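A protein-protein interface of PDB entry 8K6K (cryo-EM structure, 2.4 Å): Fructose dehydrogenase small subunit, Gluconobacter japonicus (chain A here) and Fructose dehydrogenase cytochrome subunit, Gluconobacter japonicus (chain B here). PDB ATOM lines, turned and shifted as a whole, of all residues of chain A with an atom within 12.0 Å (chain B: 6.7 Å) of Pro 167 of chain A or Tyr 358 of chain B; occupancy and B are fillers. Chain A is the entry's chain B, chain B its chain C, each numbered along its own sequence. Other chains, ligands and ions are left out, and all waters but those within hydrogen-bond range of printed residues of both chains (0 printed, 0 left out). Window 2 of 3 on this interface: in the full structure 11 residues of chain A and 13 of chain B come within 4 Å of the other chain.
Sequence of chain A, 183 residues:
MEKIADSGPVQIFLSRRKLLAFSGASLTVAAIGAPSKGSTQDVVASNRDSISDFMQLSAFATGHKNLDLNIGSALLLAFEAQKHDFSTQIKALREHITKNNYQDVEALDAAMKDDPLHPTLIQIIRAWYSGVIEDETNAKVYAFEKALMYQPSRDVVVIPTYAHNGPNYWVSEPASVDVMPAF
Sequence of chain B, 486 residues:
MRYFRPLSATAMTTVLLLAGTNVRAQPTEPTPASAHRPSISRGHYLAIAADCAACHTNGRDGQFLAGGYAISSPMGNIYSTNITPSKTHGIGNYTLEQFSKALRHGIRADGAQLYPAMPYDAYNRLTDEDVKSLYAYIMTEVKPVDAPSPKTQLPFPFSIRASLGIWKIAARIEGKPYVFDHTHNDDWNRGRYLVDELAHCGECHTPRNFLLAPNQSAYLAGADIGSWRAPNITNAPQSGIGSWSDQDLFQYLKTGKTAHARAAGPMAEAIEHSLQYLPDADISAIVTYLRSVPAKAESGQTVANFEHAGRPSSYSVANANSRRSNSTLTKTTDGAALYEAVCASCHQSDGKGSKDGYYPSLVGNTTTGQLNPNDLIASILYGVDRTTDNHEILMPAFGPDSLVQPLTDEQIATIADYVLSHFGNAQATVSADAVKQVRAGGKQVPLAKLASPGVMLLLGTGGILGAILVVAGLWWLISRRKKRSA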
ATOM      1  N   VAL A 158      13.919  10.772  -7.767  1.00  0.00           N
ATOM      2  CA  VAL A 158      13.560  11.990  -7.056  1.00  0.00           C
ATOM      3  C   VAL A 158      12.448  11.690  -6.061  1.00  0.00           C
ATOM      4  O   VAL A 158      11.524  10.921  -6.347  1.00  0.00           O
ATOM      5  CB  VAL A 158      13.136  13.080  -8.056  1.00  0.00           C
ATOM      6  CG1 VAL A 158      12.045  12.563  -8.973  1.00  0.00           C
ATOM      7  CG2 VAL A 158      12.667  14.325  -7.336  1.00  0.00           C
ATOM      8  N   PRO A 160       9.363  13.313  -5.004  1.00  0.00           N
ATOM      9  CA  PRO A 160       8.755  14.247  -5.966  1.00  0.00           C
ATOM     10  C   PRO A 160       8.798  15.732  -5.629  1.00  0.00           C
ATOM     11  O   PRO A 160       9.423  16.500  -6.364  1.00  0.00           O
ATOM     12  CB  PRO A 160       7.314  13.743  -6.042  1.00  0.00           C
ATOM     13  CG  PRO A 160       7.455  12.275  -5.867  1.00  0.00           C
ATOM     14  CD  PRO A 160       8.583  12.070  -4.886  1.00  0.00           C
ATOM     15  N   TYR A 162      10.523  17.503  -3.887  1.00  0.00           N
ATOM     16  CA  TYR A 162      11.836  18.030  -3.548  1.00  0.00           C
ATOM     17  C   TYR A 162      12.791  17.761  -4.697  1.00  0.00           C
ATOM     18  O   TYR A 162      12.923  16.619  -5.145  1.00  0.00           O
ATOM     19  CB  TYR A 162      12.356  17.408  -2.254  1.00  0.00           C
ATOM     20  CG  TYR A 162      11.523  17.766  -1.051  1.00  0.00           C
ATOM     21  CD1 TYR A 162      11.778  18.918  -0.327  1.00  0.00           C
ATOM     22  CD2 TYR A 162      10.473  16.958  -0.646  1.00  0.00           C
ATOM     23  CE1 TYR A 162      11.019  19.251   0.770  1.00  0.00           C
ATOM     24  CE2 TYR A 162       9.708  17.282   0.449  1.00  0.00           C
ATOM     25  CZ  TYR A 162       9.984  18.431   1.154  1.00  0.00           C
ATOM     26  OH  TYR A 162       9.224  18.760   2.250  1.00  0.00           O
ATOM     27  N   ALA A 163      13.459  18.809  -5.163  1.00  0.00           N
ATOM     28  CA  ALA A 163      14.237  18.729  -6.389  1.00  0.00           C
ATOM     29  C   ALA A 163      15.533  17.956  -6.189  1.00  0.00           C
ATOM     30  O   ALA A 163      16.176  18.049  -5.141  1.00  0.00           O
ATOM     31  CB  ALA A 163      14.553  20.132  -6.904  1.00  0.00           C
ATOM     32  N   HIS A 164      15.905  17.187  -7.207  1.00  0.00           N
ATOM     33  CA  HIS A 164      17.260  16.681  -7.346  1.00  0.00           C
ATOM     34  C   HIS A 164      18.157  17.811  -7.852  1.00  0.00           C
ATOM     35  O   HIS A 164      17.707  18.929  -8.110  1.00  0.00           O
ATOM     36  CB  HIS A 164      17.280  15.484  -8.290  1.00  0.00           C
ATOM     37  CG  HIS A 164      17.701  14.202  -7.645  1.00  0.00           C
ATOM     38  ND1 HIS A 164      18.785  13.472  -8.084  1.00  0.00           N
ATOM     39  CD2 HIS A 164      17.179  13.511  -6.605  1.00  0.00           C
ATOM     40  CE1 HIS A 164      18.916  12.390  -7.338  1.00  0.00           C
ATOM     41  NE2 HIS A 164      17.954  12.390  -6.432  1.00  0.00           N
ATOM     42  N   ASN A 165      19.444  17.523  -8.023  1.00  0.00           N
ATOM     43  CA  ASN A 165      20.389  18.599  -8.293  1.00  0.00           C
ATOM     44  C   ASN A 165      20.262  19.155  -9.707  1.00  0.00           C
ATOM     45  O   ASN A 165      20.889  18.648 -10.640  1.00  0.00           O
ATOM     46  CB  ASN A 165      21.824  18.124  -8.049  1.00  0.00           C
ATOM     47  CG  ASN A 165      22.137  16.824  -8.749  1.00  0.00           C
ATOM     48  OD1 ASN A 165      21.249  16.168  -9.288  1.00  0.00           O
ATOM     49  ND2 ASN A 165      23.408  16.448  -8.754  1.00  0.00           N
ATOM     50  N   GLY A 166      19.465  20.208  -9.874  1.00  0.00           N
ATOM     51  CA  GLY A 166      19.480  20.974 -11.098  1.00  0.00           C
ATOM     52  C   GLY A 166      18.336  20.679 -12.044  1.00  0.00           C
ATOM     53  O   GLY A 166      17.743  19.598 -12.031  1.00  0.00           O
ATOM     54  N   PRO A 167      18.010  21.654 -12.898  1.00  0.00           N
ATOM     55  CA  PRO A 167      16.870  21.501 -13.811  1.00  0.00           C
ATOM     56  C   PRO A 167      17.113  20.585 -14.998  1.00  0.00           C
ATOM     57  O   PRO A 167      16.223  20.472 -15.846  1.00  0.00           O
ATOM     58  CB  PRO A 167      16.613  22.939 -14.286  1.00  0.00           C
ATOM     59  CG  PRO A 167      17.240  23.796 -13.262  1.00  0.00           C
ATOM     60  CD  PRO A 167      18.456  23.050 -12.825  1.00  0.00           C
ATOM     61  N   ASN A 168      18.281  19.960 -15.134  1.00  0.00           N
ATOM     62  CA  ASN A 168      18.462  18.987 -16.206  1.00  0.00           C
ATOM     63  C   ASN A 168      19.318  17.810 -15.761  1.00  0.00           C
ATOM     64  O   ASN A 168      20.058  17.239 -16.568  1.00  0.00           O
ATOM     65  CB  ASN A 168      19.066  19.639 -17.448  1.00  0.00           C
ATOM     66  CG  ASN A 168      18.013  20.092 -18.434  1.00  0.00           C
ATOM     67  OD1 ASN A 168      17.006  19.418 -18.635  1.00  0.00           O
ATOM     68  ND2 ASN A 168      18.239  21.240 -19.058  1.00  0.00           N
ATOM     69  N   TYR A 169      19.233  17.432 -14.484  1.00  0.00           N
ATOM     70  CA  TYR A 169      20.098  16.386 -13.951  1.00  0.00           C
ATOM     71  C   TYR A 169      19.866  15.035 -14.610  1.00  0.00           C
ATOM     72  O   TYR A 169      20.771  14.195 -14.604  1.00  0.00           O
ATOM     73  CB  TYR A 169      19.894  16.259 -12.441  1.00  0.00           C
ATOM     74  CG  TYR A 169      18.583  15.617 -12.049  1.00  0.00           C
ATOM     75  CD1 TYR A 169      17.440  16.382 -11.879  1.00  0.00           C
ATOM     76  CD2 TYR A 169      18.487  14.248 -11.849  1.00  0.00           C
ATOM     77  CE1 TYR A 169      16.243  15.802 -11.526  1.00  0.00           C
ATOM     78  CE2 TYR A 169      17.295  13.661 -11.499  1.00  0.00           C
ATOM     79  CZ  TYR A 169      16.176  14.441 -11.338  1.00  0.00           C
ATOM     80  OH  TYR A 169      14.983  13.856 -10.985  1.00  0.00           O
ATOM     81  N   TRP A 170      18.684  14.803 -15.179  1.00  0.00           N
ATOM     82  CA  TRP A 170      18.322  13.466 -15.632  1.00  0.00           C
ATOM     83  C   TRP A 170      19.047  13.037 -16.898  1.00  0.00           C
ATOM     84  O   TRP A 170      18.895  11.880 -17.302  1.00  0.00           O
ATOM     85  CB  TRP A 170      16.813  13.372 -15.845  1.00  0.00           C
ATOM     86  CG  TRP A 170      16.221  14.510 -16.603  1.00  0.00           C
ATOM     87  CD1 TRP A 170      16.107  14.621 -17.954  1.00  0.00           C
ATOM     88  CD2 TRP A 170      15.643  15.694 -16.053  1.00  0.00           C
ATOM     89  NE1 TRP A 170      15.499  15.804 -18.281  1.00  0.00           N
ATOM     90  CE2 TRP A 170      15.202  16.481 -17.130  1.00  0.00           C
ATOM     91  CE3 TRP A 170      15.456  16.165 -14.754  1.00  0.00           C
ATOM     92  CZ2 TRP A 170      14.590  17.712 -16.946  1.00  0.00           C
ATOM     93  CZ3 TRP A 170      14.851  17.386 -14.576  1.00  0.00           C
ATOM     94  CH2 TRP A 170      14.419  18.143 -15.664  1.00  0.00           C
ATOM     95  N   VAL A 171      19.816  13.918 -17.538  1.00  0.00           N
ATOM     96  CA  VAL A 171      20.582  13.520 -18.712  1.00  0.00           C
ATOM     97  C   VAL A 171      21.713  12.562 -18.378  1.00  0.00           C
ATOM     98  O   VAL A 171      22.260  11.924 -19.283  1.00  0.00           O
ATOM     99  CB  VAL A 171      21.154  14.754 -19.439  1.00  0.00           C
ATOM    100  CG1 VAL A 171      20.071  15.788 -19.637  1.00  0.00           C
ATOM    101  CG2 VAL A 171      22.316  15.338 -18.662  1.00  0.00           C
ATOM    102  N   SER A 172      22.074  12.443 -17.107  1.00  0.00           N
ATOM    103  CA  SER A 172      23.145  11.556 -16.684  1.00  0.00           C
ATOM    104  C   SER A 172      22.633  10.129 -16.533  1.00  0.00           C
ATOM    105  O   SER A 172      21.447   9.886 -16.310  1.00  0.00           O
ATOM    106  CB  SER A 172      23.750  12.038 -15.366  1.00  0.00           C
ATOM    107  OG  SER A 172      22.814  11.927 -14.311  1.00  0.00           O
ATOM    108  N   LYS B 257      27.752  33.960 -10.016  1.00  0.00           N
ATOM    109  CA  LYS B 257      27.421  32.715  -9.343  1.00  0.00           C
ATOM    110  C   LYS B 257      28.642  32.223  -8.583  1.00  0.00           C
ATOM    111  O   LYS B 257      29.726  32.093  -9.158  1.00  0.00           O
ATOM    112  CB  LYS B 257      26.951  31.659 -10.346  1.00  0.00           C
ATOM    113  CG  LYS B 257      26.542  30.342  -9.722  1.00  0.00           C
ATOM    114  CD  LYS B 257      25.842  29.464 -10.739  1.00  0.00           C
ATOM    115  CE  LYS B 257      25.691  28.044 -10.235  1.00  0.00           C
ATOM    116  NZ  LYS B 257      24.744  27.270 -11.079  1.00  0.00           N
ATOM    117  N   ARG B 262      25.318  34.900  -4.726  1.00  0.00           N
ATOM    118  CA  ARG B 262      24.693  34.962  -6.039  1.00  0.00           C
ATOM    119  C   ARG B 262      24.234  36.387  -6.297  1.00  0.00           C
ATOM    120  O   ARG B 262      23.719  37.053  -5.396  1.00  0.00           O
ATOM    121  CB  ARG B 262      23.505  34.000  -6.146  1.00  0.00           C
ATOM    122  CG  ARG B 262      23.801  32.587  -5.685  1.00  0.00           C
ATOM    123  CD  ARG B 262      24.694  31.864  -6.673  1.00  0.00           C
ATOM    124  NE  ARG B 262      25.110  30.558  -6.177  1.00  0.00           N
ATOM    125  CZ  ARG B 262      24.625  29.403  -6.609  1.00  0.00           C
ATOM    126  NH1 ARG B 262      23.702  29.352  -7.554  1.00  0.00           N
ATOM    127  NH2 ARG B 262      25.077  28.272  -6.080  1.00  0.00           N
ATOM    128  N   HIS B 347      15.795  25.033  -2.544  1.00  0.00           N
ATOM    129  CA  HIS B 347      16.702  25.001  -1.405  1.00  0.00           C
ATOM    130  C   HIS B 347      16.201  23.934  -0.448  1.00  0.00           C
ATOM    131  O   HIS B 347      15.094  24.051   0.079  1.00  0.00           O
ATOM    132  CB  HIS B 347      16.762  26.355  -0.699  1.00  0.00           C
ATOM    133  CG  HIS B 347      16.745  27.530  -1.625  1.00  0.00           C
ATOM    134  ND1 HIS B 347      17.870  27.979  -2.280  1.00  0.00           N
ATOM    135  CD2 HIS B 347      15.742  28.362  -1.988  1.00  0.00           C
ATOM    136  CE1 HIS B 347      17.560  29.030  -3.015  1.00  0.00           C
ATOM    137  NE2 HIS B 347      16.274  29.283  -2.856  1.00  0.00           N
ATOM    138  N   SER B 354      20.956  22.527  -3.830  1.00  0.00           N
ATOM    139  CA  SER B 354      21.155  21.333  -4.634  1.00  0.00           C
ATOM    140  C   SER B 354      22.633  20.962  -4.691  1.00  0.00           C
ATOM    141  O   SER B 354      23.518  21.787  -4.461  1.00  0.00           O
ATOM    142  CB  SER B 354      20.607  21.539  -6.044  1.00  0.00           C
ATOM    143  OG  SER B 354      21.437  22.404  -6.793  1.00  0.00           O
ATOM    144  N   LYS B 355      22.888  19.689  -5.000  1.00  0.00           N
ATOM    145  CA  LYS B 355      24.259  19.189  -5.016  1.00  0.00           C
ATOM    146  C   LYS B 355      25.079  19.843  -6.120  1.00  0.00           C
ATOM    147  O   LYS B 355      26.259  20.154  -5.921  1.00  0.00           O
ATOM    148  CB  LYS B 355      24.263  17.671  -5.172  1.00  0.00           C
ATOM    149  CG  LYS B 355      23.782  16.931  -3.940  1.00  0.00           C
ATOM    150  CD  LYS B 355      24.404  15.550  -3.846  1.00  0.00           C
ATOM    151  CE  LYS B 355      23.491  14.587  -3.107  1.00  0.00           C
ATOM    152  NZ  LYS B 355      22.670  15.282  -2.079  1.00  0.00           N
ATOM    153  N   ASP B 356      24.479  20.059  -7.286  1.00  0.00           N
ATOM    154  CA  ASP B 356      25.191  20.672  -8.400  1.00  0.00           C
ATOM    155  C   ASP B 356      25.321  22.181  -8.259  1.00  0.00           C
ATOM    156  O   ASP B 356      25.977  22.810  -9.095  1.00  0.00           O
ATOM    157  CB  ASP B 356      24.499  20.329  -9.721  1.00  0.00           C
ATOM    158  CG  ASP B 356      23.113  20.920  -9.826  1.00  0.00           C
ATOM    159  OD1 ASP B 356      22.509  21.227  -8.779  1.00  0.00           O
ATOM    160  OD2 ASP B 356      22.625  21.077 -10.963  1.00  0.00           O
ATOM    161  N   GLY B 357      24.710  22.774  -7.239  1.00  0.00           N
ATOM    162  CA  GLY B 357      24.871  24.183  -6.965  1.00  0.00           C
ATOM    163  C   GLY B 357      23.954  25.108  -7.729  1.00  0.00           C
ATOM    164  O   GLY B 357      24.059  26.328  -7.556  1.00  0.00           O
ATOM    165  N   TYR B 358      23.063  24.578  -8.569  1.00  0.00           N
ATOM    166  CA  TYR B 358      22.129  25.444  -9.280  1.00  0.00           C
ATOM    167  C   TYR B 358      21.241  26.201  -8.305  1.00  0.00           C
ATOM    168  O   TYR B 358      21.021  27.407  -8.462  1.00  0.00           O
ATOM    169  CB  TYR B 358      21.280  24.627 -10.254  1.00  0.00           C
ATOM    170  CG  TYR B 358      20.390  25.472 -11.136  1.00  0.00           C
ATOM    171  CD1 TYR B 358      19.121  25.843 -10.723  1.00  0.00           C
ATOM    172  CD2 TYR B 358      20.821  25.902 -12.381  1.00  0.00           C
ATOM    173  CE1 TYR B 358      18.310  26.616 -11.520  1.00  0.00           C
ATOM    174  CE2 TYR B 358      20.014  26.675 -13.186  1.00  0.00           C
ATOM    175  CZ  TYR B 358      18.759  27.027 -12.751  1.00  0.00           C
ATOM    176  OH  TYR B 358      17.949  27.797 -13.548  1.00  0.00           O
ATOM    177  N   TYR B 359      20.724  25.512  -7.293  1.00  0.00           N
ATOM    178  CA  TYR B 359      19.977  26.163  -6.230  1.00  0.00           C
ATOM    179  C   TYR B 359      20.940  26.464  -5.094  1.00  0.00           C
ATOM    180  O   TYR B 359      21.484  25.525  -4.494  1.00  0.00           O
ATOM    181  CB  TYR B 359      18.835  25.282  -5.758  1.00  0.00           C
ATOM    182  CG  TYR B 359      17.838  25.012  -6.853  1.00  0.00           C
ATOM    183  CD1 TYR B 359      17.296  26.057  -7.581  1.00  0.00           C
ATOM    184  CD2 TYR B 359      17.459  23.721  -7.180  1.00  0.00           C
ATOM    185  CE1 TYR B 359      16.397  25.828  -8.589  1.00  0.00           C
ATOM    186  CE2 TYR B 359      16.554  23.483  -8.191  1.00  0.00           C
ATOM    187  CZ  TYR B 359      16.028  24.544  -8.891  1.00  0.00           C
ATOM    188  OH  TYR B 359      15.127  24.334  -9.902  1.00  0.00           O
ATOM    189  N   PRO B 360      21.193  27.729  -4.774  1.00  0.00           N
ATOM    190  CA  PRO B 360      22.264  28.051  -3.830  1.00  0.00           C
ATOM    191  C   PRO B 360      21.950  27.574  -2.425  1.00  0.00           C
ATOM    192  O   PRO B 360      20.791  27.449  -2.025  1.00  0.00           O
ATOM    193  CB  PRO B 360      22.337  29.579  -3.892  1.00  0.00           C
ATOM    194  CG  PRO B 360      20.974  29.992  -4.291  1.00  0.00           C
ATOM    195  CD  PRO B 360      20.471  28.929  -5.219  1.00  0.00           C
ATOM    196  N   HIS B 391      22.564  31.855 -20.772  1.00  0.00           N
ATOM    197  CA  HIS B 391      21.882  30.908 -19.902  1.00  0.00           C
ATOM    198  C   HIS B 391      21.272  31.681 -18.745  1.00  0.00           C
ATOM    199  O   HIS B 391      21.957  32.486 -18.106  1.00  0.00           O
ATOM    200  CB  HIS B 391      22.843  29.834 -19.386  1.00  0.00           C
ATOM    201  CG  HIS B 391      22.209  28.861 -18.443  1.00  0.00           C
ATOM    202  ND1 HIS B 391      21.155  28.051 -18.807  1.00  0.00           N
ATOM    203  CD2 HIS B 391      22.476  28.571 -17.148  1.00  0.00           C
ATOM    204  CE1 HIS B 391      20.801  27.303 -17.777  1.00  0.00           C
ATOM    205  NE2 HIS B 391      21.588  27.599 -16.760  1.00  0.00           N
ATOM    206  N   GLU B 392      19.993  31.440 -18.474  1.00  0.00           N
ATOM    207  CA  GLU B 392      19.230  32.261 -17.544  1.00  0.00           C
ATOM    208  C   GLU B 392      18.983  31.518 -16.238  1.00  0.00           C
ATOM    209  O   GLU B 392      18.363  30.450 -16.229  1.00  0.00           O
ATOM    210  CB  GLU B 392      17.903  32.692 -18.167  1.00  0.00           C
ATOM    211  CG  GLU B 392      17.293  33.916 -17.515  1.00  0.00           C
ATOM    212  CD  GLU B 392      15.895  34.205 -18.010  1.00  0.00           C
ATOM    213  OE1 GLU B 392      15.654  34.079 -19.228  1.00  0.00           O
ATOM    214  OE2 GLU B 392      15.036  34.569 -17.185  1.00  0.00           O
ATOM    215  N   ILE B 393      19.495  32.081 -15.145  1.00  0.00           N
ATOM    216  CA  ILE B 393      18.960  31.827 -13.815  1.00  0.00           C
ATOM    217  C   ILE B 393      17.563  32.415 -13.687  1.00  0.00           C
ATOM    218  O   ILE B 393      17.231  33.431 -14.313  1.00  0.00           O
ATOM    219  CB  ILE B 393      19.902  32.421 -12.751  1.00  0.00           C
ATOM    220  CG1 ILE B 393      20.856  31.366 -12.162  1.00  0.00           C
ATOM    221  CG2 ILE B 393      19.142  33.312 -11.768  1.00  0.00           C
ATOM    222  CD1 ILE B 393      21.676  30.637 -13.206  1.00  0.00           C
ATOM    223  N   LEU B 394      16.729  31.776 -12.868  1.00  0.00           N
ATOM    224  CA  LEU B 394      15.510  32.434 -12.425  1.00  0.00           C
ATOM    225  C   LEU B 394      15.045  31.866 -11.094  1.00  0.00           C
ATOM    226  O   LEU B 394      14.843  30.657 -10.960  1.00  0.00           O
ATOM    227  CB  LEU B 394      14.388  32.314 -13.458  1.00  0.00           C
ATOM    228  CG  LEU B 394      13.296  33.368 -13.262  1.00  0.00           C
ATOM    229  CD1 LEU B 394      12.942  34.020 -14.581  1.00  0.00           C
ATOM    230  CD2 LEU B 394      12.064  32.776 -12.607  1.00  0.00           C
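The backbone carbonyl oxygen (O) of Asn 165 of chain A sits close to the side-chain carboxylate (OD2) of Asp 356 of chain B.
OD1 of Asp 356 of chain B lies within hydrogen-bond range of N of Gly 166 of chain A, at 3.4 Å.
The side-chain carboxylate of Asp 356 of chain B lies close to the backbone NH of Tyr 358 of chain B.
The side-chain hydroxyl (OG) of Ser 354 of chain B sits at hydrogen-bond distance from the backbone NH (N) of Gly 357 of chain B, at 3.3 Å.
The backbone NH (N) of Ser 354 of chain B sits at hydrogen-bond distance from the backbone carbonyl oxygen (O) of Tyr 359 of chain B (3.1 Å).
N of Tyr 358 of chain B lies within hydrogen-bond range of OG of Ser 354 of chain B (3.2 Å).
The backbone carbonyl oxygen (O) of Tyr 358 of chain B sits at hydrogen-bond distance from the guanidinium group (NH1) of Arg 262 of chain B.
OG of Ser 354 of chain B sits at hydrogen-bond distance from OD1 of Asp 356 of chain B (2.5 Å).
Asn 165 of chain A touches Ser 354 of chain B (CA to CB, 3.7 Å).
Lys 355 of chain B touches Asn 165 of chain A.
CG of Pro 167 of chain A touches CE1 of Tyr 358 of chain B (3.5 Å).
Printed residues of chain B within 4 Å of Asn 165 of chain A: Ser 354 (3.7 Å), Lys 355 (3.6 Å) and Asp 356 (3.0 Å).
Of the printed residues of chain B, Gly 166 of chain A touches Asp 356.
Printed residues of chain B within 4 Å of Pro 167 of chain A: Tyr 358 (3.5 Å).
Of the printed residues of chain A, Ser 354 of chain B touches Asn 165.
Of the printed residues of chain A, Lys 355 of chain B touches Asn 165 (3.6 Å).
Asp 356 of chain B touches just these residues of chain A: Asn 165 (3.0 Å) and Gly 166 (3.1 Å).
No residue of chain A comes within 4 Å of Gly 357 of chain B.
Printed residues of chain A within 4 Å of Tyr 358 of chain B: Pro 167.
No residue of chain A comes within 4 Å of Ile 393 of chain B.
The nearest printed residue of chain A that does not touch Lys 355 of chain B is His 164 of chain A (5.8 Å).
Of the 14 printed residues of chain B, 4 touch a printed residue of chain A.
Printed residues of chain B that touch a printed residue of chain A: Ser 354, Lys 355, Asp 356 and Tyr 358.
Of the 13 printed residues of chain A, 3 touch a printed residue of chain B.
Printed residues of chain A that touch a printed residue of chain B: Asn 165, Gly 166 and Pro 167.
Among the printed residues, 5 pairs touch across the chains.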
